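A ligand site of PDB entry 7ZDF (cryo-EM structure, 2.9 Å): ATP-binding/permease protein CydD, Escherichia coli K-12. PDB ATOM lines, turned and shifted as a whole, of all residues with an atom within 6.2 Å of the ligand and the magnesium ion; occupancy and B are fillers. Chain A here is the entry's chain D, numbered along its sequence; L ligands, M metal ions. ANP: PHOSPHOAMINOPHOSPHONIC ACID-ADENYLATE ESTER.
The side-chain amino group of Lys 389 lies within hydrogen-bond range of the side-chain hydroxyl of Ser 387 (3.2 Å). The backbone carbonyl oxygen of Arg 384 sits at hydrogen-bond distance from the side-chain amino group of Lys 389 (2.9 Å). OE1 of Glu 511 is in hydrogen-bond range of NE2 of Gln 430 (2.7 Å). The backbone NH (N) of Gln 430 lies close to the backbone carbonyl oxygen (O) of Asp 510 (3.3 Å). The side-chain hydroxyl (OG) of Ser 387 lies within hydrogen-bond range of the backbone carbonyl oxygen (O) of Arg 384 (2.7 Å). The backbone NH (N) of Lys 363 is in hydrogen-bond range of the side-chain hydroxyl (OG) of Ser 359. The side-chain hydroxyl of Ser 359 sits close to the backbone NH of Glu 361 (3.3 Å). The backbone NH (N) of Glu 511 sits at hydrogen-bond distance from the backbone carbonyl oxygen (O) of Val 540.
Of the 25 residues printed, 2 come within 4 Å of the magnesium ion. The nearest printed residue that does not touch the magnesium ion is Asp 510 (4.002 Å).
The magnesium ion is bound by the side-chain hydroxyl (OG) of Ser 390, an oxygen (O2B) of the ligand and an oxygen (O2G) of the ligand. The magnesium ion has three donor atoms within binding distance. Slightly farther from the magnesium ion lies OE1 of Gln 430 (2.8 Å).
O2B of the ligand sits close to N of Ser 390, at 2.8 Å. The backbone NH (N) of Ser 391 sits at hydrogen-bond distance from an oxygen (O2A) of the ligand (3.1 Å). OG of Ser 391 is in hydrogen-bond range of O2A of the ligand (2.4 Å). N of Lys 389 is in hydrogen-bond range of O1B of the ligand (3.3 Å). An oxygen (O1B) of the ligand is in salt-bridge range of the side-chain amino group (NZ) of Lys 389. An oxygen (O2G) of the ligand sits close to the side-chain amide nitrogen (NE2) of Gln 430. The side-chain hydroxyl (OG) of Ser 385 sits at hydrogen-bond distance from an oxygen (O1G) of the ligand (2.9 Å). A nitrogen (N6) of the ligand is in hydrogen-bond range of the backbone carbonyl oxygen (O) of Ala 112 (3.0 Å). N of Gly 388 lies within hydrogen-bond range of O3A of the ligand, 3.2 Å away. The backbone NH of Gly 386 is in hydrogen-bond range of an oxygen (O1B) of the ligand (3.4 Å). N of Ser 387 sits at hydrogen-bond distance from O1B of the ligand (3.2 Å). OG of Ser 387 is in hydrogen-bond range of O1B of the ligand (3.5 Å). The side-chain amino group of Lys 363 is in hydrogen-bond range of a nitrogen (N3) of the ligand.
Residues that only touch the ligand: Leu 365, Ser 359, Arg 384 and Glu 511. Hydrophobic or aromatic side chains that line the ligand: Leu 365.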
ATOM      1  N   PRO A 111     -21.917  -9.128 -26.329  1.00  0.00           N
ATOM      2  CA  PRO A 111     -20.484  -8.942 -26.047  1.00  0.00           C
ATOM      3  C   PRO A 111     -19.624 -10.119 -26.462  1.00  0.00           C
ATOM      4  O   PRO A 111     -18.419  -9.947 -26.634  1.00  0.00           O
ATOM      5  CB  PRO A 111     -20.455  -8.757 -24.521  1.00  0.00           C
ATOM      6  CG  PRO A 111     -21.748  -9.291 -24.034  1.00  0.00           C
ATOM      7  CD  PRO A 111     -22.741  -9.061 -25.112  1.00  0.00           C
ATOM      8  N   ALA A 112     -20.206 -11.307 -26.640  1.00  0.00           N
ATOM      9  CA  ALA A 112     -19.424 -12.463 -27.047  1.00  0.00           C
ATOM     10  C   ALA A 112     -18.780 -12.246 -28.408  1.00  0.00           C
ATOM     11  O   ALA A 112     -17.698 -12.787 -28.681  1.00  0.00           O
ATOM     12  CB  ALA A 112     -20.305 -13.703 -27.064  1.00  0.00           C
ATOM     13  N   TRP A 113     -19.422 -11.475 -29.284  1.00  0.00           N
ATOM     14  CA  TRP A 113     -18.908 -11.179 -30.609  1.00  0.00           C
ATOM     15  C   TRP A 113     -18.340  -9.774 -30.746  1.00  0.00           C
ATOM     16  O   TRP A 113     -17.499  -9.546 -31.614  1.00  0.00           O
ATOM     17  CB  TRP A 113     -20.001 -11.378 -31.661  1.00  0.00           C
ATOM     18  CG  TRP A 113     -19.488 -11.492 -33.059  1.00  0.00           C
ATOM     19  CD1 TRP A 113     -18.535 -12.347 -33.515  1.00  0.00           C
ATOM     20  CD2 TRP A 113     -19.909 -10.725 -34.183  1.00  0.00           C
ATOM     21  NE1 TRP A 113     -18.331 -12.158 -34.851  1.00  0.00           N
ATOM     22  CE2 TRP A 113     -19.163 -11.163 -35.289  1.00  0.00           C
ATOM     23  CE3 TRP A 113     -20.848  -9.702 -34.361  1.00  0.00           C
ATOM     24  CZ2 TRP A 113     -19.324 -10.618 -36.564  1.00  0.00           C
ATOM     25  CZ3 TRP A 113     -21.008  -9.164 -35.625  1.00  0.00           C
ATOM     26  CH2 TRP A 113     -20.249  -9.622 -36.710  1.00  0.00           C
ATOM     27  N   SER A 359     -18.663 -20.525 -28.773  1.00  0.00           N
ATOM     28  CA  SER A 359     -18.491 -19.166 -29.252  1.00  0.00           C
ATOM     29  C   SER A 359     -19.532 -18.856 -30.322  1.00  0.00           C
ATOM     30  O   SER A 359     -20.144 -19.764 -30.884  1.00  0.00           O
ATOM     31  CB  SER A 359     -17.076 -18.983 -29.805  1.00  0.00           C
ATOM     32  OG  SER A 359     -16.998 -19.422 -31.150  1.00  0.00           O
ATOM     33  N   PRO A 360     -19.773 -17.574 -30.602  1.00  0.00           N
ATOM     34  CA  PRO A 360     -20.731 -17.227 -31.670  1.00  0.00           C
ATOM     35  C   PRO A 360     -20.335 -17.779 -33.029  1.00  0.00           C
ATOM     36  O   PRO A 360     -21.207 -18.018 -33.873  1.00  0.00           O
ATOM     37  CB  PRO A 360     -20.741 -15.694 -31.660  1.00  0.00           C
ATOM     38  CG  PRO A 360     -20.284 -15.333 -30.290  1.00  0.00           C
ATOM     39  CD  PRO A 360     -19.250 -16.357 -29.943  1.00  0.00           C
ATOM     40  N   GLU A 361     -19.041 -17.981 -33.280  1.00  0.00           N
ATOM     41  CA  GLU A 361     -18.575 -18.564 -34.527  1.00  0.00           C
ATOM     42  C   GLU A 361     -18.676 -20.086 -34.544  1.00  0.00           C
ATOM     43  O   GLU A 361     -18.380 -20.695 -35.570  1.00  0.00           O
ATOM     44  CB  GLU A 361     -17.131 -18.133 -34.801  1.00  0.00           C
ATOM     45  CG  GLU A 361     -16.951 -16.656 -35.054  1.00  0.00           C
ATOM     46  CD  GLU A 361     -17.613 -16.193 -36.343  1.00  0.00           C
ATOM     47  OE1 GLU A 361     -17.671 -16.993 -37.298  1.00  0.00           O
ATOM     48  OE2 GLU A 361     -18.057 -15.027 -36.396  1.00  0.00           O
ATOM     49  N   LYS A 363     -17.033 -22.233 -32.344  1.00  0.00           N
ATOM     50  CA  LYS A 363     -15.935 -22.888 -31.647  1.00  0.00           C
ATOM     51  C   LYS A 363     -16.335 -23.239 -30.218  1.00  0.00           C
ATOM     52  O   LYS A 363     -17.067 -22.487 -29.560  1.00  0.00           O
ATOM     53  CB  LYS A 363     -14.697 -21.984 -31.646  1.00  0.00           C
ATOM     54  CG  LYS A 363     -13.533 -22.506 -30.839  1.00  0.00           C
ATOM     55  CD  LYS A 363     -12.363 -21.543 -30.883  1.00  0.00           C
ATOM     56  CE  LYS A 363     -11.620 -21.509 -29.555  1.00  0.00           C
ATOM     57  NZ  LYS A 363     -10.698 -20.345 -29.478  1.00  0.00           N
ATOM     58  N   THR A 364     -15.860 -24.389 -29.744  1.00  0.00           N
ATOM     59  CA  THR A 364     -16.124 -24.819 -28.384  1.00  0.00           C
ATOM     60  C   THR A 364     -15.131 -24.158 -27.441  1.00  0.00           C
ATOM     61  O   THR A 364     -13.918 -24.320 -27.598  1.00  0.00           O
ATOM     62  CB  THR A 364     -16.037 -26.339 -28.275  1.00  0.00           C
ATOM     63  OG1 THR A 364     -17.170 -26.925 -28.929  1.00  0.00           O
ATOM     64  CG2 THR A 364     -16.023 -26.780 -26.824  1.00  0.00           C
ATOM     65  N   LEU A 365     -15.647 -23.420 -26.452  1.00  0.00           N
ATOM     66  CA  LEU A 365     -14.800 -22.674 -25.534  1.00  0.00           C
ATOM     67  C   LEU A 365     -14.429 -23.483 -24.301  1.00  0.00           C
ATOM     68  O   LEU A 365     -13.248 -23.591 -23.956  1.00  0.00           O
ATOM     69  CB  LEU A 365     -15.492 -21.374 -25.135  1.00  0.00           C
ATOM     70  CG  LEU A 365     -15.829 -20.442 -26.297  1.00  0.00           C
ATOM     71  CD1 LEU A 365     -16.457 -19.159 -25.803  1.00  0.00           C
ATOM     72  CD2 LEU A 365     -14.587 -20.164 -27.116  1.00  0.00           C
ATOM     73  N   GLY A 383      -7.468 -21.447 -12.335  1.00  0.00           N
ATOM     74  CA  GLY A 383      -6.814 -22.142 -13.418  1.00  0.00           C
ATOM     75  C   GLY A 383      -5.854 -21.224 -14.141  1.00  0.00           C
ATOM     76  O   GLY A 383      -5.673 -20.062 -13.774  1.00  0.00           O
ATOM     77  N   ARG A 384      -5.255 -21.776 -15.202  1.00  0.00           N
ATOM     78  CA  ARG A 384      -4.297 -21.048 -16.055  1.00  0.00           C
ATOM     79  C   ARG A 384      -5.083 -20.189 -17.054  1.00  0.00           C
ATOM     80  O   ARG A 384      -6.289 -20.413 -17.209  1.00  0.00           O
ATOM     81  CB  ARG A 384      -3.368 -22.036 -16.763  1.00  0.00           C
ATOM     82  CG  ARG A 384      -2.340 -22.672 -15.854  1.00  0.00           C
ATOM     83  CD  ARG A 384      -2.082 -24.135 -16.161  1.00  0.00           C
ATOM     84  NE  ARG A 384      -1.876 -24.377 -17.583  1.00  0.00           N
ATOM     85  CZ  ARG A 384      -1.770 -25.587 -18.129  1.00  0.00           C
ATOM     86  NH1 ARG A 384      -1.853 -26.658 -17.374  1.00  0.00           N
ATOM     87  NH2 ARG A 384      -1.578 -25.704 -19.427  1.00  0.00           N
ATOM     88  N   SER A 385      -4.402 -19.228 -17.666  1.00  0.00           N
ATOM     89  CA  SER A 385      -5.040 -18.342 -18.629  1.00  0.00           C
ATOM     90  C   SER A 385      -5.529 -19.135 -19.836  1.00  0.00           C
ATOM     91  O   SER A 385      -4.871 -20.075 -20.291  1.00  0.00           O
ATOM     92  CB  SER A 385      -4.066 -17.256 -19.079  1.00  0.00           C
ATOM     93  OG  SER A 385      -4.709 -16.288 -19.878  1.00  0.00           O
ATOM     94  N   GLY A 386      -6.692 -18.752 -20.356  1.00  0.00           N
ATOM     95  CA  GLY A 386      -7.256 -19.440 -21.497  1.00  0.00           C
ATOM     96  C   GLY A 386      -7.867 -20.788 -21.176  1.00  0.00           C
ATOM     97  O   GLY A 386      -7.962 -21.642 -22.062  1.00  0.00           O
ATOM     98  N   SER A 387      -8.264 -21.009 -19.933  1.00  0.00           N
ATOM     99  CA  SER A 387      -8.855 -22.278 -19.516  1.00  0.00           C
ATOM    100  C   SER A 387     -10.372 -22.249 -19.517  1.00  0.00           C
ATOM    101  O   SER A 387     -10.996 -23.231 -19.100  1.00  0.00           O
ATOM    102  CB  SER A 387      -8.348 -22.658 -18.121  1.00  0.00           C
ATOM    103  OG  SER A 387      -8.634 -21.649 -17.177  1.00  0.00           O
ATOM    104  N   GLY A 388     -10.981 -21.162 -19.982  1.00  0.00           N
ATOM    105  CA  GLY A 388     -12.425 -21.083 -20.063  1.00  0.00           C
ATOM    106  C   GLY A 388     -13.121 -20.586 -18.816  1.00  0.00           C
ATOM    107  O   GLY A 388     -14.303 -20.884 -18.638  1.00  0.00           O
ATOM    108  N   LYS A 389     -12.422 -19.860 -17.946  1.00  0.00           N
ATOM    109  CA  LYS A 389     -13.052 -19.384 -16.715  1.00  0.00           C
ATOM    110  C   LYS A 389     -14.034 -18.250 -16.990  1.00  0.00           C
ATOM    111  O   LYS A 389     -15.096 -18.189 -16.370  1.00  0.00           O
ATOM    112  CB  LYS A 389     -11.976 -18.937 -15.729  1.00  0.00           C
ATOM    113  CG  LYS A 389     -11.017 -20.040 -15.320  1.00  0.00           C
ATOM    114  CD  LYS A 389     -10.003 -19.542 -14.326  1.00  0.00           C
ATOM    115  CE  LYS A 389      -9.234 -18.354 -14.855  1.00  0.00           C
ATOM    116  NZ  LYS A 389      -8.336 -18.735 -15.982  1.00  0.00           N
ATOM    117  N   SER A 390     -13.694 -17.358 -17.920  1.00  0.00           N
ATOM    118  CA  SER A 390     -14.610 -16.238 -18.247  1.00  0.00           C
ATOM    119  C   SER A 390     -15.759 -16.736 -19.129  1.00  0.00           C
ATOM    120  O   SER A 390     -16.811 -16.089 -19.123  1.00  0.00           O
ATOM    121  CB  SER A 390     -13.906 -15.075 -18.888  1.00  0.00           C
ATOM    122  OG  SER A 390     -13.348 -14.229 -17.899  1.00  0.00           O
ATOM    123  N   SER A 391     -15.540 -17.819 -19.867  1.00  0.00           N
ATOM    124  CA  SER A 391     -16.609 -18.375 -20.695  1.00  0.00           C
ATOM    125  C   SER A 391     -17.739 -18.927 -19.830  1.00  0.00           C
ATOM    126  O   SER A 391     -18.911 -18.797 -20.179  1.00  0.00           O
ATOM    127  CB  SER A 391     -16.055 -19.466 -21.599  1.00  0.00           C
ATOM    128  OG  SER A 391     -14.955 -18.989 -22.344  1.00  0.00           O
ATOM    129  N   LEU A 392     -17.395 -19.553 -18.700  1.00  0.00           N
ATOM    130  CA  LEU A 392     -18.424 -20.082 -17.808  1.00  0.00           C
ATOM    131  C   LEU A 392     -19.248 -18.954 -17.211  1.00  0.00           C
ATOM    132  O   LEU A 392     -20.462 -19.100 -17.005  1.00  0.00           O
ATOM    133  CB  LEU A 392     -17.780 -20.927 -16.714  1.00  0.00           C
ATOM    134  CG  LEU A 392     -18.728 -21.593 -15.725  1.00  0.00           C
ATOM    135  CD1 LEU A 392     -19.847 -22.318 -16.455  1.00  0.00           C
ATOM    136  CD2 LEU A 392     -17.983 -22.553 -14.827  1.00  0.00           C
ATOM    137  N   ASN A 394     -19.638 -15.955 -18.732  1.00  0.00           N
ATOM    138  CA  ASN A 394     -20.379 -15.367 -19.846  1.00  0.00           C
ATOM    139  C   ASN A 394     -21.561 -16.238 -20.249  1.00  0.00           C
ATOM    140  O   ASN A 394     -22.593 -15.717 -20.674  1.00  0.00           O
ATOM    141  CB  ASN A 394     -19.456 -15.141 -21.039  1.00  0.00           C
ATOM    142  CG  ASN A 394     -18.384 -14.122 -20.765  1.00  0.00           C
ATOM    143  OD1 ASN A 394     -18.559 -13.221 -19.948  1.00  0.00           O
ATOM    144  ND2 ASN A 394     -17.258 -14.240 -21.454  1.00  0.00           N
ATOM    145  N   LEU A 400     -23.331 -16.498 -24.098  1.00  0.00           N
ATOM    146  CA  LEU A 400     -22.791 -17.593 -24.888  1.00  0.00           C
ATOM    147  C   LEU A 400     -23.797 -18.737 -24.926  1.00  0.00           C
ATOM    148  O   LEU A 400     -24.536 -18.964 -23.970  1.00  0.00           O
ATOM    149  CB  LEU A 400     -21.462 -18.096 -24.306  1.00  0.00           C
ATOM    150  CG  LEU A 400     -20.263 -17.163 -24.519  1.00  0.00           C
ATOM    151  CD1 LEU A 400     -19.079 -17.641 -23.718  1.00  0.00           C
ATOM    152  CD2 LEU A 400     -19.923 -17.094 -25.990  1.00  0.00           C
ATOM    153  N   GLN A 430     -14.093  -8.612 -15.996  1.00  0.00           N
ATOM    154  CA  GLN A 430     -12.641  -8.470 -15.891  1.00  0.00           C
ATOM    155  C   GLN A 430     -12.196  -7.033 -16.127  1.00  0.00           C
ATOM    156  O   GLN A 430     -11.280  -6.546 -15.466  1.00  0.00           O
ATOM    157  CB  GLN A 430     -11.965  -9.421 -16.880  1.00  0.00           C
ATOM    158  CG  GLN A 430     -10.564  -9.851 -16.463  1.00  0.00           C
ATOM    159  CD  GLN A 430     -10.089 -11.058 -17.236  1.00  0.00           C
ATOM    160  OE1 GLN A 430     -10.841 -11.678 -17.975  1.00  0.00           O
ATOM    161  NE2 GLN A 430      -8.808 -11.396 -17.073  1.00  0.00           N
ATOM    162  N   ASP A 510     -15.465 -11.721 -12.134  1.00  0.00           N
ATOM    163  CA  ASP A 510     -14.476 -12.188 -13.101  1.00  0.00           C
ATOM    164  C   ASP A 510     -13.170 -11.438 -12.841  1.00  0.00           C
ATOM    165  O   ASP A 510     -12.967 -10.338 -13.369  1.00  0.00           O
ATOM    166  CB  ASP A 510     -14.973 -11.971 -14.527  1.00  0.00           C
ATOM    167  CG  ASP A 510     -14.376 -12.957 -15.502  1.00  0.00           C
ATOM    168  OD1 ASP A 510     -13.282 -13.485 -15.231  1.00  0.00           O
ATOM    169  OD2 ASP A 510     -15.006 -13.198 -16.554  1.00  0.00           O
ATOM    170  N   GLU A 511     -12.281 -12.049 -12.068  1.00  0.00           N
ATOM    171  CA  GLU A 511     -11.014 -11.476 -11.640  1.00  0.00           C
ATOM    172  C   GLU A 511     -11.171  -9.998 -11.270  1.00  0.00           C
ATOM    173  O   GLU A 511     -10.561  -9.128 -11.893  1.00  0.00           O
ATOM    174  CB  GLU A 511      -9.940 -11.650 -12.707  1.00  0.00           C
ATOM    175  CG  GLU A 511      -9.533 -13.107 -12.918  1.00  0.00           C
ATOM    176  CD  GLU A 511      -8.481 -13.290 -13.989  1.00  0.00           C
ATOM    177  OE1 GLU A 511      -8.137 -12.302 -14.672  1.00  0.00           O
ATOM    178  OE2 GLU A 511      -7.984 -14.427 -14.143  1.00  0.00           O
ATOM    179  N   VAL A 540     -14.086 -15.715 -10.171  1.00  0.00           N
ATOM    180  CA  VAL A 540     -12.858 -16.122 -10.847  1.00  0.00           C
ATOM    181  C   VAL A 540     -11.723 -15.279 -10.294  1.00  0.00           C
ATOM    182  O   VAL A 540     -11.863 -14.058 -10.144  1.00  0.00           O
ATOM    183  CB  VAL A 540     -12.973 -15.945 -12.369  1.00  0.00           C
ATOM    184  CG1 VAL A 540     -11.706 -16.405 -13.046  1.00  0.00           C
ATOM    185  CG2 VAL A 540     -14.150 -16.721 -12.898  1.00  0.00           C
HETATM  186  PG  ANP L   1      -8.016 -15.314 -18.787  1.00  0.00           P
HETATM  187  O1G ANP L   1      -7.041 -14.535 -19.609  1.00  0.00           O
HETATM  188  O2G ANP L   1      -9.031 -14.375 -18.195  1.00  0.00           O
HETATM  189  O3G ANP L   1      -7.258 -15.958 -17.666  1.00  0.00           O
HETATM  190  PB  ANP L   1      -9.977 -17.401 -19.229  1.00  0.00           P
HETATM  191  O1B ANP L   1      -9.450 -18.496 -18.353  1.00  0.00           O
HETATM  192  O2B ANP L   1     -11.141 -16.588 -18.732  1.00  0.00           O
HETATM  193  N3B ANP L   1      -8.777 -16.422 -19.709  1.00  0.00           N
HETATM  194  PA  ANP L   1     -11.575 -17.618 -21.657  1.00  0.00           P
HETATM  195  O1A ANP L   1     -11.533 -16.129 -21.724  1.00  0.00           O
HETATM  196  O2A ANP L   1     -12.871 -18.277 -21.344  1.00  0.00           O
HETATM  197  O3A ANP L   1     -10.479 -18.087 -20.585  1.00  0.00           O
HETATM  198  O5' ANP L   1     -10.989 -18.217 -23.018  1.00  0.00           O
HETATM  199  C5' ANP L   1     -10.997 -19.641 -23.267  1.00  0.00           C
HETATM  200  C4' ANP L   1     -10.471 -19.896 -24.668  1.00  0.00           C
HETATM  201  O4' ANP L   1     -11.492 -19.508 -25.618  1.00  0.00           O
HETATM  202  C3' ANP L   1      -9.268 -19.039 -25.057  1.00  0.00           C
HETATM  203  O3' ANP L   1      -8.603 -19.598 -26.182  1.00  0.00           O
HETATM  204  C2' ANP L   1      -9.960 -17.747 -25.479  1.00  0.00           C
HETATM  205  O2' ANP L   1      -9.164 -16.865 -26.225  1.00  0.00           O
HETATM  206  C1' ANP L   1     -11.101 -18.338 -26.301  1.00  0.00           C
HETATM  207  N9  ANP L   1     -12.276 -17.480 -26.404  1.00  0.00           N
HETATM  208  C8  ANP L   1     -12.865 -16.770 -25.397  1.00  0.00           C
HETATM  209  N7  ANP L   1     -13.918 -16.095 -25.812  1.00  0.00           N
HETATM  210  C5  ANP L   1     -13.994 -16.371 -27.169  1.00  0.00           C
HETATM  211  C6  ANP L   1     -14.891 -15.942 -28.174  1.00  0.00           C
HETATM  212  N6  ANP L   1     -15.916 -15.132 -27.948  1.00  0.00           N
HETATM  213  N1  ANP L   1     -14.684 -16.421 -29.416  1.00  0.00           N
HETATM  214  C2  ANP L   1     -13.657 -17.252 -29.629  1.00  0.00           C
HETATM  215  N3  ANP L   1     -12.755 -17.707 -28.772  1.00  0.00           N
HETATM  216  C4  ANP L   1     -12.986 -17.223 -27.535  1.00  0.00           C
HETATM  217 MG    MG M   1     -11.234 -14.376 -18.552  1.00  0.00          MG
